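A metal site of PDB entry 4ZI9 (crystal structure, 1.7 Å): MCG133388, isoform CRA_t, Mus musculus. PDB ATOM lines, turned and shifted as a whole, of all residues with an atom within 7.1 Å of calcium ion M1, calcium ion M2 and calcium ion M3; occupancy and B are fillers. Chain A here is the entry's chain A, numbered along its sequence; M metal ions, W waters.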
ATOM      1  N   GLU A 117      -7.986  -9.844  15.244  1.00  0.00           N
ATOM      2  CA  GLU A 117      -6.670  -9.740  15.857  1.00  0.00           C
ATOM      3  C   GLU A 117      -6.653 -10.276  17.284  1.00  0.00           C
ATOM      4  O   GLU A 117      -5.562 -10.550  17.828  1.00  0.00           O
ATOM      5  CB  GLU A 117      -6.158  -8.301  15.806  1.00  0.00           C
ATOM      6  CG  GLU A 117      -7.080  -7.253  16.422  1.00  0.00           C
ATOM      7  CD  GLU A 117      -6.440  -5.892  16.410  1.00  0.00           C
ATOM      8  OE1 GLU A 117      -7.169  -4.894  16.279  1.00  0.00           O
ATOM      9  OE2 GLU A 117      -5.196  -5.835  16.523  1.00  0.00           O
ATOM     10  N   LEU A 173      -1.989 -12.170  16.768  1.00  0.00           N
ATOM     11  CA  LEU A 173      -2.090 -11.224  15.671  1.00  0.00           C
ATOM     12  C   LEU A 173      -2.214  -9.776  16.163  1.00  0.00           C
ATOM     13  O   LEU A 173      -2.547  -9.530  17.327  1.00  0.00           O
ATOM     14  CB  LEU A 173      -3.291 -11.576  14.807  1.00  0.00           C
ATOM     15  CG  LEU A 173      -3.268 -13.006  14.260  1.00  0.00           C
ATOM     16  CD1 LEU A 173      -4.592 -13.263  13.580  1.00  0.00           C
ATOM     17  CD2 LEU A 173      -2.104 -13.164  13.282  1.00  0.00           C
ATOM     18  N   ASP A 174      -1.935  -8.813  15.275  1.00  0.00           N
ATOM     19  CA  ASP A 174      -2.103  -7.388  15.596  1.00  0.00           C
ATOM     20  C   ASP A 174      -2.302  -6.612  14.314  1.00  0.00           C
ATOM     21  O   ASP A 174      -1.352  -6.383  13.571  1.00  0.00           O
ATOM     22  CB  ASP A 174      -0.909  -6.837  16.367  1.00  0.00           C
ATOM     23  CG  ASP A 174      -1.022  -5.338  16.644  1.00  0.00           C
ATOM     24  OD1 ASP A 174      -2.085  -4.717  16.433  1.00  0.00           O
ATOM     25  OD2 ASP A 174      -0.018  -4.753  17.087  1.00  0.00           O
ATOM     26  N   ARG A 175      -3.545  -6.230  14.023  1.00  0.00           N
ATOM     27  CA  ARG A 175      -3.849  -5.497  12.794  1.00  0.00           C
ATOM     28  C   ARG A 175      -3.064  -4.188  12.678  1.00  0.00           C
ATOM     29  O   ARG A 175      -2.754  -3.765  11.577  1.00  0.00           O
ATOM     30  CB  ARG A 175      -5.344  -5.212  12.724  1.00  0.00           C
ATOM     31  CG  ARG A 175      -5.873  -4.862  11.343  1.00  0.00           C
ATOM     32  CD  ARG A 175      -7.078  -3.964  11.461  1.00  0.00           C
ATOM     33  NE  ARG A 175      -6.692  -2.702  12.108  1.00  0.00           N
ATOM     34  CZ  ARG A 175      -6.286  -1.622  11.454  1.00  0.00           C
ATOM     35  NH1 ARG A 175      -6.260  -1.613  10.121  1.00  0.00           N
ATOM     36  NH2 ARG A 175      -5.927  -0.539  12.115  1.00  0.00           N
ATOM     37  N   GLU A 176      -2.746  -3.546  13.806  1.00  0.00           N
ATOM     38  CA  GLU A 176      -1.990  -2.300  13.746  1.00  0.00           C
ATOM     39  C   GLU A 176      -0.508  -2.530  13.378  1.00  0.00           C
ATOM     40  O   GLU A 176       0.200  -1.584  13.049  1.00  0.00           O
ATOM     41  CB  GLU A 176      -2.086  -1.539  15.080  1.00  0.00           C
ATOM     42  CG  GLU A 176      -3.407  -0.849  15.288  1.00  0.00           C
ATOM     43  CD  GLU A 176      -4.575  -1.808  15.557  1.00  0.00           C
ATOM     44  OE1 GLU A 176      -4.449  -2.718  16.414  1.00  0.00           O
ATOM     45  OE2 GLU A 176      -5.648  -1.610  14.950  1.00  0.00           O
ATOM     46  N   LYS A 177      -0.062  -3.778  13.404  1.00  0.00           N
ATOM     47  CA  LYS A 177       1.287  -4.116  12.908  1.00  0.00           C
ATOM     48  C   LYS A 177       1.180  -4.713  11.508  1.00  0.00           C
ATOM     49  O   LYS A 177       1.817  -4.252  10.573  1.00  0.00           O
ATOM     50  CB  LYS A 177       1.988  -5.093  13.860  1.00  0.00           C
ATOM     51  CG  LYS A 177       3.418  -5.476  13.471  1.00  0.00           C
ATOM     52  CD  LYS A 177       3.987  -6.562  14.402  1.00  0.00           C
ATOM     53  CE  LYS A 177       5.521  -6.655  14.343  1.00  0.00           C
ATOM     54  NZ  LYS A 177       6.038  -7.103  13.023  1.00  0.00           N
ATOM     55  N   VAL A 206      -8.899  -8.922  11.232  1.00  0.00           N
ATOM     56  CA  VAL A 206     -10.059  -8.091  11.513  1.00  0.00           C
ATOM     57  C   VAL A 206      -9.804  -7.220  12.750  1.00  0.00           C
ATOM     58  O   VAL A 206      -9.249  -7.666  13.765  1.00  0.00           O
ATOM     59  CB  VAL A 206     -11.321  -8.943  11.695  1.00  0.00           C
ATOM     60  CG1 VAL A 206     -12.506  -8.057  11.910  1.00  0.00           C
ATOM     61  CG2 VAL A 206     -11.545  -9.770  10.452  1.00  0.00           C
ATOM     62  N   ASP A 207     -10.163  -5.951  12.630  1.00  0.00           N
ATOM     63  CA  ASP A 207      -9.851  -4.982  13.679  1.00  0.00           C
ATOM     64  C   ASP A 207     -10.610  -5.250  14.980  1.00  0.00           C
ATOM     65  O   ASP A 207     -11.765  -5.694  14.949  1.00  0.00           O
ATOM     66  CB  ASP A 207     -10.150  -3.553  13.185  1.00  0.00           C
ATOM     67  CG  ASP A 207      -9.653  -2.465  14.159  1.00  0.00           C
ATOM     68  OD1 ASP A 207      -8.540  -2.574  14.716  1.00  0.00           O
ATOM     69  OD2 ASP A 207     -10.399  -1.509  14.381  1.00  0.00           O
ATOM     70  N   VAL A 208      -9.943  -5.008  16.101  1.00  0.00           N
ATOM     71  CA  VAL A 208     -10.607  -4.865  17.407  1.00  0.00           C
ATOM     72  C   VAL A 208     -10.294  -3.459  17.934  1.00  0.00           C
ATOM     73  O   VAL A 208      -9.199  -2.938  17.683  1.00  0.00           O
ATOM     74  CB  VAL A 208     -10.124  -5.942  18.403  1.00  0.00           C
ATOM     75  CG1 VAL A 208     -10.653  -5.672  19.817  1.00  0.00           C
ATOM     76  CG2 VAL A 208     -10.539  -7.351  17.917  1.00  0.00           C
ATOM     77  N   ASN A 209     -11.230  -2.829  18.658  1.00  0.00           N
ATOM     78  CA  ASN A 209     -10.904  -1.534  19.247  1.00  0.00           C
ATOM     79  C   ASN A 209      -9.991  -1.778  20.430  1.00  0.00           C
ATOM     80  O   ASN A 209     -10.467  -1.871  21.557  1.00  0.00           O
ATOM     81  CB  ASN A 209     -12.143  -0.772  19.693  1.00  0.00           C
ATOM     82  CG  ASN A 209     -11.815   0.688  20.019  1.00  0.00           C
ATOM     83  OD1 ASN A 209     -10.871   1.276  19.434  1.00  0.00           O
ATOM     84  ND2 ASN A 209     -12.559   1.279  20.957  1.00  0.00           N
ATOM     85  N   ASP A 210      -8.705  -1.880  20.187  1.00  0.00           N
ATOM     86  CA  ASP A 210      -7.792  -2.197  21.281  1.00  0.00           C
ATOM     87  C   ASP A 210      -6.742  -1.109  21.523  1.00  0.00           C
ATOM     88  O   ASP A 210      -5.737  -1.339  22.214  1.00  0.00           O
ATOM     89  CB  ASP A 210      -7.135  -3.577  21.071  1.00  0.00           C
ATOM     90  CG  ASP A 210      -6.374  -3.712  19.747  1.00  0.00           C
ATOM     91  OD1 ASP A 210      -6.626  -2.968  18.765  1.00  0.00           O
ATOM     92  OD2 ASP A 210      -5.508  -4.609  19.685  1.00  0.00           O
ATOM     93  N   ASN A 211      -6.966   0.071  20.960  1.00  0.00           N
ATOM     94  CA  ASN A 211      -6.118   1.229  21.251  1.00  0.00           C
ATOM     95  C   ASN A 211      -6.994   2.405  21.628  1.00  0.00           C
ATOM     96  O   ASN A 211      -7.941   2.720  20.913  1.00  0.00           O
ATOM     97  CB  ASN A 211      -5.253   1.647  20.068  1.00  0.00           C
ATOM     98  CG  ASN A 211      -4.265   0.584  19.656  1.00  0.00           C
ATOM     99  OD1 ASN A 211      -3.117   0.589  20.089  1.00  0.00           O
ATOM    100  ND2 ASN A 211      -4.717  -0.351  18.820  1.00  0.00           N
ATOM    101  N   PRO A 212      -6.682   3.051  22.750  1.00  0.00           N
ATOM    102  CA  PRO A 212      -7.334   4.322  23.061  1.00  0.00           C
ATOM    103  C   PRO A 212      -6.764   5.443  22.198  1.00  0.00           C
ATOM    104  O   PRO A 212      -5.661   5.342  21.694  1.00  0.00           O
ATOM    105  CB  PRO A 212      -6.984   4.540  24.528  1.00  0.00           C
ATOM    106  CG  PRO A 212      -5.579   3.995  24.600  1.00  0.00           C
ATOM    107  CD  PRO A 212      -5.607   2.743  23.712  1.00  0.00           C
ATOM    108  N   PRO A 213      -7.518   6.539  22.044  1.00  0.00           N
ATOM    109  CA  PRO A 213      -6.873   7.699  21.407  1.00  0.00           C
ATOM    110  C   PRO A 213      -5.686   8.205  22.253  1.00  0.00           C
ATOM    111  O   PRO A 213      -5.503   7.795  23.396  1.00  0.00           O
ATOM    112  CB  PRO A 213      -7.987   8.743  21.345  1.00  0.00           C
ATOM    113  CG  PRO A 213      -9.262   8.005  21.656  1.00  0.00           C
ATOM    114  CD  PRO A 213      -8.894   6.811  22.466  1.00  0.00           C
ATOM    115  N   THR A 240      -4.793  11.145  18.188  1.00  0.00           N
ATOM    116  CA  THR A 240      -4.725  10.161  17.110  1.00  0.00           C
ATOM    117  C   THR A 240      -5.135   8.805  17.665  1.00  0.00           C
ATOM    118  O   THR A 240      -5.105   8.588  18.879  1.00  0.00           O
ATOM    119  CB  THR A 240      -3.327  10.088  16.517  1.00  0.00           C
ATOM    120  OG1 THR A 240      -2.373   9.817  17.548  1.00  0.00           O
ATOM    121  CG2 THR A 240      -2.963  11.410  15.848  1.00  0.00           C
ATOM    122  N   ASP A 241      -5.520   7.890  16.772  1.00  0.00           N
ATOM    123  CA  ASP A 241      -6.017   6.574  17.177  1.00  0.00           C
ATOM    124  C   ASP A 241      -5.775   5.599  16.017  1.00  0.00           C
ATOM    125  O   ASP A 241      -6.278   5.815  14.920  1.00  0.00           O
ATOM    126  CB  ASP A 241      -7.483   6.625  17.531  1.00  0.00           C
ATOM    127  CG  ASP A 241      -7.986   5.335  18.176  1.00  0.00           C
ATOM    128  OD1 ASP A 241      -7.622   4.214  17.723  1.00  0.00           O
ATOM    129  OD2 ASP A 241      -8.744   5.453  19.160  1.00  0.00           O
ATOM    130  N   PRO A 242      -4.985   4.549  16.256  1.00  0.00           N
ATOM    131  CA  PRO A 242      -4.504   3.688  15.165  1.00  0.00           C
ATOM    132  C   PRO A 242      -5.481   2.572  14.753  1.00  0.00           C
ATOM    133  O   PRO A 242      -5.189   1.836  13.823  1.00  0.00           O
ATOM    134  CB  PRO A 242      -3.226   3.099  15.748  1.00  0.00           C
ATOM    135  CG  PRO A 242      -3.497   3.049  17.218  1.00  0.00           C
ATOM    136  CD  PRO A 242      -4.362   4.216  17.548  1.00  0.00           C
ATOM    137  N   ASP A 243      -6.603   2.441  15.436  1.00  0.00           N
ATOM    138  CA  ASP A 243      -7.589   1.438  15.052  1.00  0.00           C
ATOM    139  C   ASP A 243      -8.307   1.857  13.769  1.00  0.00           C
ATOM    140  O   ASP A 243      -8.139   2.992  13.287  1.00  0.00           O
ATOM    141  CB  ASP A 243      -8.604   1.200  16.186  1.00  0.00           C
ATOM    142  CG  ASP A 243      -7.960   0.619  17.419  1.00  0.00           C
ATOM    143  OD1 ASP A 243      -7.169  -0.339  17.305  1.00  0.00           O
ATOM    144  OD2 ASP A 243      -8.206   1.161  18.496  1.00  0.00           O
ATOM    145  N   GLU A 244      -9.117   0.947  13.229  1.00  0.00           N
ATOM    146  CA  GLU A 244      -9.720   1.104  11.904  1.00  0.00           C
ATOM    147  C   GLU A 244     -11.144   1.656  11.967  1.00  0.00           C
ATOM    148  O   GLU A 244     -11.934   1.282  12.831  1.00  0.00           O
ATOM    149  CB  GLU A 244      -9.726  -0.244  11.170  1.00  0.00           C
ATOM    150  CG  GLU A 244     -10.355  -0.217   9.780  1.00  0.00           C
ATOM    151  CD  GLU A 244     -10.297  -1.578   9.066  1.00  0.00           C
ATOM    152  OE1 GLU A 244     -10.237  -2.612   9.762  1.00  0.00           O
ATOM    153  OE2 GLU A 244     -10.290  -1.605   7.824  1.00  0.00           O
ATOM    154  N   ALA A 246     -14.512   3.430  12.624  1.00  0.00           N
ATOM    155  CA  ALA A 246     -15.095   4.038  13.811  1.00  0.00           C
ATOM    156  C   ALA A 246     -14.228   3.836  15.052  1.00  0.00           C
ATOM    157  O   ALA A 246     -14.227   4.689  15.949  1.00  0.00           O
ATOM    158  CB  ALA A 246     -16.474   3.492  14.047  1.00  0.00           C
ATOM    159  N   ASN A 247     -13.524   2.718  15.106  1.00  0.00           N
ATOM    160  CA  ASN A 247     -12.623   2.437  16.234  1.00  0.00           C
ATOM    161  C   ASN A 247     -11.466   3.433  16.372  1.00  0.00           C
ATOM    162  O   ASN A 247     -10.903   3.580  17.466  1.00  0.00           O
ATOM    163  CB  ASN A 247     -12.066   1.018  16.120  1.00  0.00           C
ATOM    164  CG  ASN A 247     -13.143  -0.026  16.136  1.00  0.00           C
ATOM    165  OD1 ASN A 247     -14.215   0.191  16.694  1.00  0.00           O
ATOM    166  ND2 ASN A 247     -12.863  -1.186  15.544  1.00  0.00           N
ATOM    167  N   GLY A 248     -11.112   4.086  15.268  1.00  0.00           N
ATOM    168  CA  GLY A 248     -10.028   5.062  15.236  1.00  0.00           C
ATOM    169  C   GLY A 248     -10.499   6.506  15.025  1.00  0.00           C
ATOM    170  O   GLY A 248      -9.688   7.423  14.868  1.00  0.00           O
ATOM    171  N   ARG A 249     -11.810   6.694  14.988  1.00  0.00           N
ATOM    172  CA  ARG A 249     -12.386   8.024  14.770  1.00  0.00           C
ATOM    173  C   ARG A 249     -12.667   8.705  16.108  1.00  0.00           C
ATOM    174  O   ARG A 249     -13.434   8.194  16.930  1.00  0.00           O
ATOM    175  CB  ARG A 249     -13.681   7.896  13.950  1.00  0.00           C
ATOM    176  CG  ARG A 249     -14.339   9.199  13.536  1.00  0.00           C
ATOM    177  CD  ARG A 249     -15.358   8.903  12.438  1.00  0.00           C
ATOM    178  NE  ARG A 249     -14.799   8.032  11.400  1.00  0.00           N
ATOM    179  CZ  ARG A 249     -15.301   6.851  11.032  1.00  0.00           C
ATOM    180  NH1 ARG A 249     -16.392   6.371  11.616  1.00  0.00           N
ATOM    181  NH2 ARG A 249     -14.702   6.150  10.069  1.00  0.00           N
ATOM    182  N   VAL A 250     -12.047   9.859  16.337  1.00  0.00           N
ATOM    183  CA  VAL A 250     -12.138  10.459  17.663  1.00  0.00           C
ATOM    184  C   VAL A 250     -12.890  11.783  17.688  1.00  0.00           C
ATOM    185  O   VAL A 250     -12.808  12.609  16.768  1.00  0.00           O
ATOM    186  CB  VAL A 250     -10.726  10.642  18.286  1.00  0.00           C
ATOM    187  CG1 VAL A 250      -9.680   9.923  17.471  1.00  0.00           C
ATOM    188  CG2 VAL A 250     -10.370  12.084  18.477  1.00  0.00           C
ATOM    189  N   ASP A 296     -12.880   7.568  21.085  1.00  0.00           N
ATOM    190  CA  ASP A 296     -13.010   6.922  19.774  1.00  0.00           C
ATOM    191  C   ASP A 296     -14.469   6.475  19.622  1.00  0.00           C
ATOM    192  O   ASP A 296     -15.308   6.787  20.447  1.00  0.00           O
ATOM    193  CB  ASP A 296     -12.031   5.744  19.585  1.00  0.00           C
ATOM    194  CG  ASP A 296     -12.249   4.600  20.567  1.00  0.00           C
ATOM    195  OD1 ASP A 296     -13.377   4.376  21.092  1.00  0.00           O
ATOM    196  OD2 ASP A 296     -11.248   3.881  20.799  1.00  0.00           O
ATOM    197  N   GLY A 297     -14.764   5.732  18.565  1.00  0.00           N
ATOM    198  CA  GLY A 297     -16.152   5.421  18.310  1.00  0.00           C
ATOM    199  C   GLY A 297     -16.661   4.198  19.048  1.00  0.00           C
ATOM    200  O   GLY A 297     -17.787   3.773  18.812  1.00  0.00           O
ATOM    201  N   ALA A 298     -15.857   3.639  19.955  1.00  0.00           N
ATOM    202  CA  ALA A 298     -16.241   2.365  20.581  1.00  0.00           C
ATOM    203  C   ALA A 298     -15.783   2.232  22.038  1.00  0.00           C
ATOM    204  O   ALA A 298     -15.364   1.145  22.453  1.00  0.00           O
ATOM    205  CB  ALA A 298     -15.712   1.170  19.740  1.00  0.00           C
ATOM    206  N   LEU A 300     -13.290   3.759  24.022  1.00  0.00           N
ATOM    207  CA  LEU A 300     -11.988   4.019  24.616  1.00  0.00           C
ATOM    208  C   LEU A 300     -11.753   5.530  24.585  1.00  0.00           C
ATOM    209  O   LEU A 300     -12.307   6.249  23.763  1.00  0.00           O
ATOM    210  CB  LEU A 300     -10.866   3.258  23.902  1.00  0.00           C
ATOM    211  CG  LEU A 300     -10.906   1.732  24.034  1.00  0.00           C
ATOM    212  CD1 LEU A 300      -9.740   1.137  23.294  1.00  0.00           C
ATOM    213  CD2 LEU A 300     -10.874   1.326  25.508  1.00  0.00           C
HETATM  214 CA    CA M   1      -9.433   3.095  19.176  1.00  0.00          CA
HETATM  215 CA    CA M   2      -7.086  -2.577  16.495  1.00  0.00          CA
HETATM  216 CA    CA M   3      -3.857  -4.377  17.855  1.00  0.00          CA
HETATM  217  O   HOH W   1      -2.909  -6.113  19.129  1.00  0.00           O
HETATM  218  O   HOH W   2      -2.837  -2.729  19.367  1.00  0.00           O
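Within 4 Å of calcium ion M3: Glu 117, Asp 174, Glu 176 and Asp 210.
Within 4 Å of calcium ion M1: Asn 209, Asn 211, Asp 241, Asp 243, Asn 247 and Asp 296.
The nearest printed residue that does not touch calcium ion M1 is Gly 248 (4.4 Å).
Calcium ion M2 is bound by the side-chain carboxylate (OD1) of Asp 207 (2.3 Å), the side-chain carboxylate (OE2) of Glu 176 (2.3 Å), the side-chain carboxylate (OE1) of Glu 117 (2.3 Å), the side-chain carboxylate (OD1) of Asp 210 (2.3 Å), the side-chain carboxylate (OD1) of Asp 243 (2.4 Å), the backbone carbonyl oxygen (O) of Val 208 (2.5 Å) and the side-chain carboxylate (OE1) of Glu 176 (2.6 Å).
OE1 of Glu 176 sits close to ND2 of Asn 211, 3.4 Å away.
OE2 of Glu 176 lies close to NH2 of Arg 175, 3.0 Å away.
The side-chain amide nitrogen (ND2) of Asn 247 sits at hydrogen-bond distance from the side-chain carboxylate (OD2) of Asp 207 (2.7 Å).
The side-chain carboxylate of Asp 207 sits close to the guanidinium group of Arg 175.
The backbone NH of Glu 244 sits at hydrogen-bond distance from the side-chain carboxylate of Asp 207 (3.0 Å).
The side-chain carboxylate (OE2) of Glu 117 lies close to the backbone NH (N) of Arg 175 (3.0 Å).
ND2 of Asn 209 sits at hydrogen-bond distance from O of Ala 298, at 3.2 Å.
OD1 of Asp 296 lies within hydrogen-bond range of N of Ala 298 (2.8 Å).
Calcium ion M3 is bound by OE1 of Glu 176 (2.3 Å), OD1 of Asp 174 (2.3 Å), water W1 (2.4 Å), OE2 of Glu 117 (2.4 Å), water W2 (2.5 Å) and OD2 of Asp 210 (2.5 Å).
Calcium ion M3 has six donor atoms within binding distance.
Calcium ion M1 is bound by O of Asn 247 (2.3 Å), O of Asn 211 (2.3 Å), OD1 of Asn 209 (2.3 Å), OD2 of Asp 243 (2.4 Å), OD2 of Asp 241 (2.5 Å), OD2 of Asp 296 (2.6 Å) and OD1 of Asp 241 (2.6 Å).
Calcium ion M1 has seven donor atoms within binding distance.
Within 4 Å of calcium ion M2: Glu 117, Glu 176, Asp 207, Val 208, Asp 210, Asn 211 and Asp 243.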
